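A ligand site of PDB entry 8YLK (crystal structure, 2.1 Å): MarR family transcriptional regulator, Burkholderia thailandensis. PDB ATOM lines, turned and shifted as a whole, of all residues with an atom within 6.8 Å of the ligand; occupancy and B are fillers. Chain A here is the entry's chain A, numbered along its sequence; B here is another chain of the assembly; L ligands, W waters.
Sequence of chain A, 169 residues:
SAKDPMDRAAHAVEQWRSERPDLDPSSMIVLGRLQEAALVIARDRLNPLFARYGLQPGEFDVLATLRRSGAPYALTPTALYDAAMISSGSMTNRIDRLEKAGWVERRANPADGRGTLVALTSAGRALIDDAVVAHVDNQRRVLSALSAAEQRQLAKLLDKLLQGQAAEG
O1 of the ligand sits at hydrogen-bond distance from NE1 of Trp 16 of chain B (2.5 Å). The guanidinium group (NE) of Arg 68 sits at hydrogen-bond distance from an oxygen (O1) of the ligand (2.8 Å). The side-chain carboxylate of Asp 61 is in hydrogen-bond range of a nitrogen (N3) of the ligand (2.9 Å). NE2 of His 135 lies within hydrogen-bond range of O2 of the ligand. N1 of the ligand sits at hydrogen-bond distance from SD of Met 28 of chain B (3.4 Å).
Merely in contact with the ligand: Phe 60 (3.8 Å), Ala 64 (3.4 Å), Met 85 (3.4 Å), Ile 86 (3.8 Å) and Gln 139 (3.6 Å). Hydrophobic or aromatic side chains that line the ligand: Phe 60, Ala 64, Met 85, Ile 86, His 135, Trp 16 of chain B and Met 28 of chain B. Within 4 Å of the ligand: Phe 60, Asp 61, Ala 64, Arg 68, Met 85, Ile 86, His 135, Gln 139, Trp 16 of chain B and Met 28 of chain B.
NE1 of Trp 16 of chain B sits close to SD of Met 28 of chain B (3.8 Å). NH2 of Arg 68 is in salt-bridge range of OD1 of Asp 61, at 3.99 Å. The guanidinium group (NH2) of Arg 68 is in hydrogen-bond range of the side-chain hydroxyl (OG1) of Thr 65 (3.1 Å). The guanidinium group of Arg 68 is in hydrogen-bond range of the backbone carbonyl oxygen of Ala 83 (3.0 Å). N of Met 85 is in hydrogen-bond range of OD1 of Asp 61 (3.0 Å). The side-chain carboxylate of Asp 61 sits at hydrogen-bond distance from the backbone NH of Ile 86 (3.1 Å). O of Asp 61 sits at hydrogen-bond distance from OG1 of Thr 65, 2.7 Å away. The backbone NH (N) of Met 28 of chain B sits close to the side-chain amide nitrogen (NE2) of Gln 139 (3.3 Å).
Water W1 lies within hydrogen-bond range of O3 of the ligand and NE2 of Gln 35 of chain B.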
ATOM      1  N   LEU A  46      14.902  -9.076 -13.992  1.00  0.00           N
ATOM      2  CA  LEU A  46      15.744  -8.852 -12.815  1.00  0.00           C
ATOM      3  C   LEU A  46      17.220  -8.827 -13.169  1.00  0.00           C
ATOM      4  O   LEU A  46      17.941  -7.891 -12.822  1.00  0.00           O
ATOM      5  CB  LEU A  46      15.464  -9.921 -11.758  1.00  0.00           C
ATOM      6  CG  LEU A  46      14.018 -10.010 -11.251  1.00  0.00           C
ATOM      7  CD1 LEU A  46      13.889 -11.078 -10.178  1.00  0.00           C
ATOM      8  CD2 LEU A  46      13.572  -8.656 -10.735  1.00  0.00           C
ATOM      9  N   PHE A  50      20.559  -6.215 -12.596  1.00  0.00           N
ATOM     10  CA  PHE A  50      21.780  -6.566 -11.880  1.00  0.00           C
ATOM     11  C   PHE A  50      22.999  -6.412 -12.786  1.00  0.00           C
ATOM     12  O   PHE A  50      24.075  -5.999 -12.337  1.00  0.00           O
ATOM     13  CB  PHE A  50      21.709  -7.994 -11.344  1.00  0.00           C
ATOM     14  CG  PHE A  50      20.546  -8.234 -10.424  1.00  0.00           C
ATOM     15  CD1 PHE A  50      20.080  -7.243  -9.575  1.00  0.00           C
ATOM     16  CD2 PHE A  50      19.908  -9.471 -10.399  1.00  0.00           C
ATOM     17  CE1 PHE A  50      19.017  -7.474  -8.732  1.00  0.00           C
ATOM     18  CE2 PHE A  50      18.843  -9.710  -9.569  1.00  0.00           C
ATOM     19  CZ  PHE A  50      18.391  -8.711  -8.726  1.00  0.00           C
ATOM     20  N   GLY A  58      22.808 -14.004  -8.824  1.00  0.00           N
ATOM     21  CA  GLY A  58      23.064 -14.472  -7.482  1.00  0.00           C
ATOM     22  C   GLY A  58      24.053 -13.650  -6.699  1.00  0.00           C
ATOM     23  O   GLY A  58      24.111 -13.781  -5.471  1.00  0.00           O
ATOM     24  N   PHE A  60      23.977 -10.309  -6.471  1.00  0.00           N
ATOM     25  CA  PHE A  60      23.150  -9.332  -5.785  1.00  0.00           C
ATOM     26  C   PHE A  60      22.686  -9.858  -4.428  1.00  0.00           C
ATOM     27  O   PHE A  60      22.764  -9.146  -3.414  1.00  0.00           O
ATOM     28  CB  PHE A  60      21.935  -8.987  -6.654  1.00  0.00           C
ATOM     29  CG  PHE A  60      20.983  -7.993  -6.030  1.00  0.00           C
ATOM     30  CD1 PHE A  60      21.161  -6.627  -6.215  1.00  0.00           C
ATOM     31  CD2 PHE A  60      19.895  -8.430  -5.290  1.00  0.00           C
ATOM     32  CE1 PHE A  60      20.279  -5.709  -5.659  1.00  0.00           C
ATOM     33  CE2 PHE A  60      19.012  -7.529  -4.725  1.00  0.00           C
ATOM     34  CZ  PHE A  60      19.198  -6.160  -4.904  1.00  0.00           C
ATOM     35  N   ASP A  61      22.220 -11.108  -4.391  1.00  0.00           N
ATOM     36  CA  ASP A  61      21.711 -11.683  -3.146  1.00  0.00           C
ATOM     37  C   ASP A  61      22.768 -11.641  -2.050  1.00  0.00           C
ATOM     38  O   ASP A  61      22.472 -11.275  -0.908  1.00  0.00           O
ATOM     39  CB  ASP A  61      21.246 -13.115  -3.392  1.00  0.00           C
ATOM     40  CG  ASP A  61      20.334 -13.647  -2.294  1.00  0.00           C
ATOM     41  OD1 ASP A  61      19.914 -12.859  -1.414  1.00  0.00           O
ATOM     42  OD2 ASP A  61      20.009 -14.858  -2.318  1.00  0.00           O
ATOM     43  N   VAL A  62      24.021 -11.982  -2.380  1.00  0.00           N
ATOM     44  CA  VAL A  62      25.089 -11.943  -1.390  1.00  0.00           C
ATOM     45  C   VAL A  62      25.267 -10.542  -0.836  1.00  0.00           C
ATOM     46  O   VAL A  62      25.324 -10.337   0.378  1.00  0.00           O
ATOM     47  CB  VAL A  62      26.407 -12.477  -1.999  1.00  0.00           C
ATOM     48  CG1 VAL A  62      27.539 -12.336  -0.985  1.00  0.00           C
ATOM     49  CG2 VAL A  62      26.270 -13.929  -2.457  1.00  0.00           C
ATOM     50  N   ALA A  64      23.086  -7.999  -1.000  1.00  0.00           N
ATOM     51  CA  ALA A  64      21.869  -7.596  -0.310  1.00  0.00           C
ATOM     52  C   ALA A  64      21.765  -8.248   1.059  1.00  0.00           C
ATOM     53  O   ALA A  64      21.361  -7.600   2.038  1.00  0.00           O
ATOM     54  CB  ALA A  64      20.640  -7.937  -1.157  1.00  0.00           C
ATOM     55  N   THR A  65      22.138  -9.527   1.165  1.00  0.00           N
ATOM     56  CA  THR A  65      22.064 -10.215   2.452  1.00  0.00           C
ATOM     57  C   THR A  65      23.038  -9.595   3.447  1.00  0.00           C
ATOM     58  O   THR A  65      22.680  -9.351   4.609  1.00  0.00           O
ATOM     59  CB  THR A  65      22.357 -11.700   2.261  1.00  0.00           C
ATOM     60  OG1 THR A  65      21.385 -12.274   1.371  1.00  0.00           O
ATOM     61  CG2 THR A  65      22.283 -12.434   3.589  1.00  0.00           C
ATOM     62  N   ARG A  68      21.629  -5.878   4.511  1.00  0.00           N
ATOM     63  CA  ARG A  68      20.506  -5.812   5.428  1.00  0.00           C
ATOM     64  C   ARG A  68      20.755  -6.565   6.731  1.00  0.00           C
ATOM     65  O   ARG A  68      19.872  -6.551   7.598  1.00  0.00           O
ATOM     66  CB  ARG A  68      19.226  -6.327   4.758  1.00  0.00           C
ATOM     67  CG  ARG A  68      19.285  -7.778   4.341  1.00  0.00           C
ATOM     68  CD  ARG A  68      17.956  -8.207   3.737  1.00  0.00           C
ATOM     69  NE  ARG A  68      18.130  -9.247   2.733  1.00  0.00           N
ATOM     70  CZ  ARG A  68      18.319 -10.537   3.006  1.00  0.00           C
ATOM     71  NH1 ARG A  68      18.370 -10.964   4.259  1.00  0.00           N
ATOM     72  NH2 ARG A  68      18.469 -11.401   2.007  1.00  0.00           N
ATOM     73  N   ALA A  83      20.462 -16.583   5.559  1.00  0.00           N
ATOM     74  CA  ALA A  83      19.789 -15.309   5.397  1.00  0.00           C
ATOM     75  C   ALA A  83      19.591 -14.922   3.936  1.00  0.00           C
ATOM     76  O   ALA A  83      18.966 -13.897   3.659  1.00  0.00           O
ATOM     77  CB  ALA A  83      20.560 -14.198   6.122  1.00  0.00           C
ATOM     78  N   ALA A  84      20.113 -15.721   3.005  1.00  0.00           N
ATOM     79  CA  ALA A  84      19.930 -15.435   1.590  1.00  0.00           C
ATOM     80  C   ALA A  84      18.450 -15.437   1.224  1.00  0.00           C
ATOM     81  O   ALA A  84      17.641 -16.145   1.831  1.00  0.00           O
ATOM     82  CB  ALA A  84      20.680 -16.452   0.742  1.00  0.00           C
ATOM     83  N   MET A  85      18.089 -14.618   0.235  1.00  0.00           N
ATOM     84  CA  MET A  85      16.724 -14.620  -0.264  1.00  0.00           C
ATOM     85  C   MET A  85      16.402 -15.922  -1.003  1.00  0.00           C
ATOM     86  O   MET A  85      15.285 -16.446  -0.896  1.00  0.00           O
ATOM     87  CB  MET A  85      16.489 -13.422  -1.179  1.00  0.00           C
ATOM     88  CG  MET A  85      15.158 -13.472  -1.925  1.00  0.00           C
ATOM     89  SD  MET A  85      13.752 -13.115  -0.862  1.00  0.00           S
ATOM     90  CE  MET A  85      13.945 -11.349  -0.618  1.00  0.00           C
ATOM     91  N   ILE A  86      17.356 -16.442  -1.765  1.00  0.00           N
ATOM     92  CA  ILE A  86      17.175 -17.614  -2.607  1.00  0.00           C
ATOM     93  C   ILE A  86      18.250 -18.642  -2.254  1.00  0.00           C
ATOM     94  O   ILE A  86      19.436 -18.309  -2.186  1.00  0.00           O
ATOM     95  CB  ILE A  86      17.250 -17.251  -4.106  1.00  0.00           C
ATOM     96  CG1 ILE A  86      16.317 -16.076  -4.409  1.00  0.00           C
ATOM     97  CG2 ILE A  86      16.880 -18.432  -4.962  1.00  0.00           C
ATOM     98  CD1 ILE A  86      16.333 -15.637  -5.859  1.00  0.00           C
ATOM     99  N   VAL A 132      19.917  -1.579  -4.785  1.00  0.00           N
ATOM    100  CA  VAL A 132      18.668  -2.047  -4.198  1.00  0.00           C
ATOM    101  C   VAL A 132      17.536  -1.069  -4.483  1.00  0.00           C
ATOM    102  O   VAL A 132      16.380  -1.480  -4.668  1.00  0.00           O
ATOM    103  CB  VAL A 132      18.847  -2.316  -2.693  1.00  0.00           C
ATOM    104  CG1 VAL A 132      19.034  -1.031  -1.914  1.00  0.00           C
ATOM    105  CG2 VAL A 132      17.664  -3.113  -2.156  1.00  0.00           C
ATOM    106  N   HIS A 135      16.539  -1.809  -7.869  1.00  0.00           N
ATOM    107  CA  HIS A 135      15.966  -3.146  -7.874  1.00  0.00           C
ATOM    108  C   HIS A 135      14.485  -3.113  -7.501  1.00  0.00           C
ATOM    109  O   HIS A 135      13.652  -3.685  -8.211  1.00  0.00           O
ATOM    110  CB  HIS A 135      16.738  -4.039  -6.918  1.00  0.00           C
ATOM    111  CG  HIS A 135      16.113  -5.384  -6.715  1.00  0.00           C
ATOM    112  ND1 HIS A 135      15.901  -6.268  -7.743  1.00  0.00           N
ATOM    113  CD2 HIS A 135      15.646  -5.983  -5.593  1.00  0.00           C
ATOM    114  CE1 HIS A 135      15.337  -7.363  -7.271  1.00  0.00           C
ATOM    115  NE2 HIS A 135      15.163  -7.210  -5.966  1.00  0.00           N
ATOM    116  N   VAL A 136      14.143  -2.466  -6.393  1.00  0.00           N
ATOM    117  CA  VAL A 136      12.750  -2.494  -5.936  1.00  0.00           C
ATOM    118  C   VAL A 136      11.860  -1.706  -6.887  1.00  0.00           C
ATOM    119  O   VAL A 136      10.693  -2.063  -7.100  1.00  0.00           O
ATOM    120  CB  VAL A 136      12.644  -1.967  -4.489  1.00  0.00           C
ATOM    121  CG1 VAL A 136      13.382  -2.889  -3.546  1.00  0.00           C
ATOM    122  CG2 VAL A 136      13.171  -0.548  -4.384  1.00  0.00           C
ATOM    123  N   GLN A 139      11.224  -4.063  -9.564  1.00  0.00           N
ATOM    124  CA  GLN A 139      10.296  -5.112  -9.148  1.00  0.00           C
ATOM    125  C   GLN A 139       8.843  -4.656  -9.225  1.00  0.00           C
ATOM    126  O   GLN A 139       7.974  -5.398  -9.689  1.00  0.00           O
ATOM    127  CB  GLN A 139      10.621  -5.592  -7.738  1.00  0.00           C
ATOM    128  CG  GLN A 139      11.886  -6.431  -7.625  1.00  0.00           C
ATOM    129  CD  GLN A 139      11.915  -7.273  -6.359  1.00  0.00           C
ATOM    130  OE1 GLN A 139      12.384  -8.415  -6.368  1.00  0.00           O
ATOM    131  NE2 GLN A 139      11.413  -6.708  -5.270  1.00  0.00           N
ATOM    132  N   ALA B  12      13.802 -11.200   5.076  1.00  0.00           N
ATOM    133  CA  ALA B  12      14.588 -10.239   4.324  1.00  0.00           C
ATOM    134  C   ALA B  12      13.910  -8.870   4.290  1.00  0.00           C
ATOM    135  O   ALA B  12      14.545  -7.847   4.539  1.00  0.00           O
ATOM    136  CB  ALA B  12      14.841 -10.754   2.913  1.00  0.00           C
ATOM    137  N   VAL B  13      12.615  -8.845   3.969  1.00  0.00           N
ATOM    138  CA  VAL B  13      11.868  -7.593   3.945  1.00  0.00           C
ATOM    139  C   VAL B  13      11.855  -6.947   5.327  1.00  0.00           C
ATOM    140  O   VAL B  13      11.971  -5.727   5.469  1.00  0.00           O
ATOM    141  CB  VAL B  13      10.439  -7.828   3.414  1.00  0.00           C
ATOM    142  CG1 VAL B  13       9.503  -6.706   3.858  1.00  0.00           C
ATOM    143  CG2 VAL B  13      10.457  -7.916   1.903  1.00  0.00           C
ATOM    144  N   TRP B  16      15.131  -5.169   5.734  1.00  0.00           N
ATOM    145  CA  TRP B  16      15.249  -3.964   4.906  1.00  0.00           C
ATOM    146  C   TRP B  16      14.509  -2.794   5.537  1.00  0.00           C
ATOM    147  O   TRP B  16      15.027  -1.664   5.575  1.00  0.00           O
ATOM    148  CB  TRP B  16      14.721  -4.242   3.497  1.00  0.00           C
ATOM    149  CG  TRP B  16      15.736  -4.872   2.606  1.00  0.00           C
ATOM    150  CD1 TRP B  16      15.628  -6.073   1.964  1.00  0.00           C
ATOM    151  CD2 TRP B  16      17.014  -4.340   2.240  1.00  0.00           C
ATOM    152  NE1 TRP B  16      16.765  -6.316   1.224  1.00  0.00           N
ATOM    153  CE2 TRP B  16      17.629  -5.264   1.380  1.00  0.00           C
ATOM    154  CE3 TRP B  16      17.702  -3.165   2.560  1.00  0.00           C
ATOM    155  CZ2 TRP B  16      18.898  -5.060   0.837  1.00  0.00           C
ATOM    156  CZ3 TRP B  16      18.964  -2.956   2.024  1.00  0.00           C
ATOM    157  CH2 TRP B  16      19.542  -3.898   1.171  1.00  0.00           C
ATOM    158  N   PRO B  25      10.092  -2.076   0.337  1.00  0.00           N
ATOM    159  CA  PRO B  25      10.532  -3.401  -0.128  1.00  0.00           C
ATOM    160  C   PRO B  25       9.396  -4.403  -0.261  1.00  0.00           C
ATOM    161  O   PRO B  25       9.643  -5.616  -0.276  1.00  0.00           O
ATOM    162  CB  PRO B  25      11.522  -3.837   0.948  1.00  0.00           C
ATOM    163  CG  PRO B  25      10.949  -3.220   2.207  1.00  0.00           C
ATOM    164  CD  PRO B  25      10.290  -1.916   1.790  1.00  0.00           C
ATOM    165  N   SER B  27       7.526  -5.397  -2.667  1.00  0.00           N
ATOM    166  CA  SER B  27       7.544  -6.269  -3.836  1.00  0.00           C
ATOM    167  C   SER B  27       8.497  -7.442  -3.693  1.00  0.00           C
ATOM    168  O   SER B  27       8.408  -8.404  -4.478  1.00  0.00           O
ATOM    169  CB  SER B  27       7.930  -5.454  -5.071  1.00  0.00           C
ATOM    170  OG  SER B  27       9.240  -4.962  -4.931  1.00  0.00           O
ATOM    171  N   MET B  28       9.413  -7.413  -2.714  1.00  0.00           N
ATOM    172  CA  MET B  28      10.390  -8.480  -2.584  1.00  0.00           C
ATOM    173  C   MET B  28       9.754  -9.799  -2.172  1.00  0.00           C
ATOM    174  O   MET B  28      10.257 -10.868  -2.561  1.00  0.00           O
ATOM    175  CB  MET B  28      11.457  -8.098  -1.554  1.00  0.00           C
ATOM    176  CG  MET B  28      12.361  -6.951  -1.963  1.00  0.00           C
ATOM    177  SD  MET B  28      13.488  -6.558  -0.622  1.00  0.00           S
ATOM    178  CE  MET B  28      14.658  -5.474  -1.446  1.00  0.00           C
ATOM    179  N   ILE B  29       8.669  -9.773  -1.403  1.00  0.00           N
ATOM    180  CA  ILE B  29       8.104 -11.002  -0.865  1.00  0.00           C
ATOM    181  C   ILE B  29       7.582 -11.889  -1.989  1.00  0.00           C
ATOM    182  O   ILE B  29       7.952 -13.067  -2.092  1.00  0.00           O
ATOM    183  CB  ILE B  29       6.998 -10.681   0.162  1.00  0.00           C
ATOM    184  CG1 ILE B  29       7.600 -10.008   1.382  1.00  0.00           C
ATOM    185  CG2 ILE B  29       6.252 -11.945   0.560  1.00  0.00           C
ATOM    186  CD1 ILE B  29       6.576  -9.463   2.345  1.00  0.00           C
ATOM    187  N   LEU B  31       7.997 -11.828  -5.332  1.00  0.00           N
ATOM    188  CA  LEU B  31       8.972 -12.265  -6.331  1.00  0.00           C
ATOM    189  C   LEU B  31      10.070 -13.127  -5.721  1.00  0.00           C
ATOM    190  O   LEU B  31      10.622 -14.006  -6.401  1.00  0.00           O
ATOM    191  CB  LEU B  31       9.580 -11.058  -7.050  1.00  0.00           C
ATOM    192  CG  LEU B  31       8.663 -10.235  -7.960  1.00  0.00           C
ATOM    193  CD1 LEU B  31       9.389  -9.019  -8.508  1.00  0.00           C
ATOM    194  CD2 LEU B  31       8.135 -11.090  -9.109  1.00  0.00           C
ATOM    195  N   GLY B  32      10.422 -12.888  -4.458  1.00  0.00           N
ATOM    196  CA  GLY B  32      11.359 -13.775  -3.785  1.00  0.00           C
ATOM    197  C   GLY B  32      10.756 -15.156  -3.541  1.00  0.00           C
ATOM    198  O   GLY B  32      11.423 -16.171  -3.716  1.00  0.00           O
ATOM    199  N   GLN B  35      10.612 -17.028  -6.969  1.00  0.00           N
ATOM    200  CA  GLN B  35      11.868 -17.621  -7.422  1.00  0.00           C
ATOM    201  C   GLN B  35      12.282 -18.784  -6.530  1.00  0.00           C
ATOM    202  O   GLN B  35      12.759 -19.809  -7.028  1.00  0.00           O
ATOM    203  CB  GLN B  35      12.956 -16.558  -7.471  1.00  0.00           C
ATOM    204  CG  GLN B  35      12.689 -15.446  -8.481  1.00  0.00           C
ATOM    205  CD  GLN B  35      13.841 -14.461  -8.603  1.00  0.00           C
ATOM    206  OE1 GLN B  35      14.733 -14.642  -9.419  1.00  0.00           O
ATOM    207  NE2 GLN B  35      13.820 -13.420  -7.787  1.00  0.00           N
HETATM  208  N1  LIG L   1      15.847  -8.788  -1.646  1.00  0.00           N
HETATM  209  C1  LIG L   1      16.960  -9.105  -0.899  1.00  0.00           C
HETATM  210  C2  LIG L   1      15.574  -9.280  -2.921  1.00  0.00           C
HETATM  211  N2  LIG L   1      17.879  -9.964  -1.428  1.00  0.00           N
HETATM  212  O1  LIG L   1      17.137  -8.622   0.209  1.00  0.00           O
HETATM  213  C3  LIG L   1      17.691 -10.503  -2.658  1.00  0.00           C
HETATM  214  C4  LIG L   1      16.557 -10.179  -3.414  1.00  0.00           C
HETATM  215  N3  LIG L   1      18.446 -11.370  -3.401  1.00  0.00           N
HETATM  216  O2  LIG L   1      14.530  -8.943  -3.502  1.00  0.00           O
HETATM  217  N4  LIG L   1      16.650 -10.868  -4.598  1.00  0.00           N
HETATM  218  C5  LIG L   1      17.802 -11.599  -4.590  1.00  0.00           C
HETATM  219  O3  LIG L   1      18.203 -12.337  -5.504  1.00  0.00           O
HETATM  220  O   HOH W   1      16.775 -12.525  -8.212  1.00  0.00           O
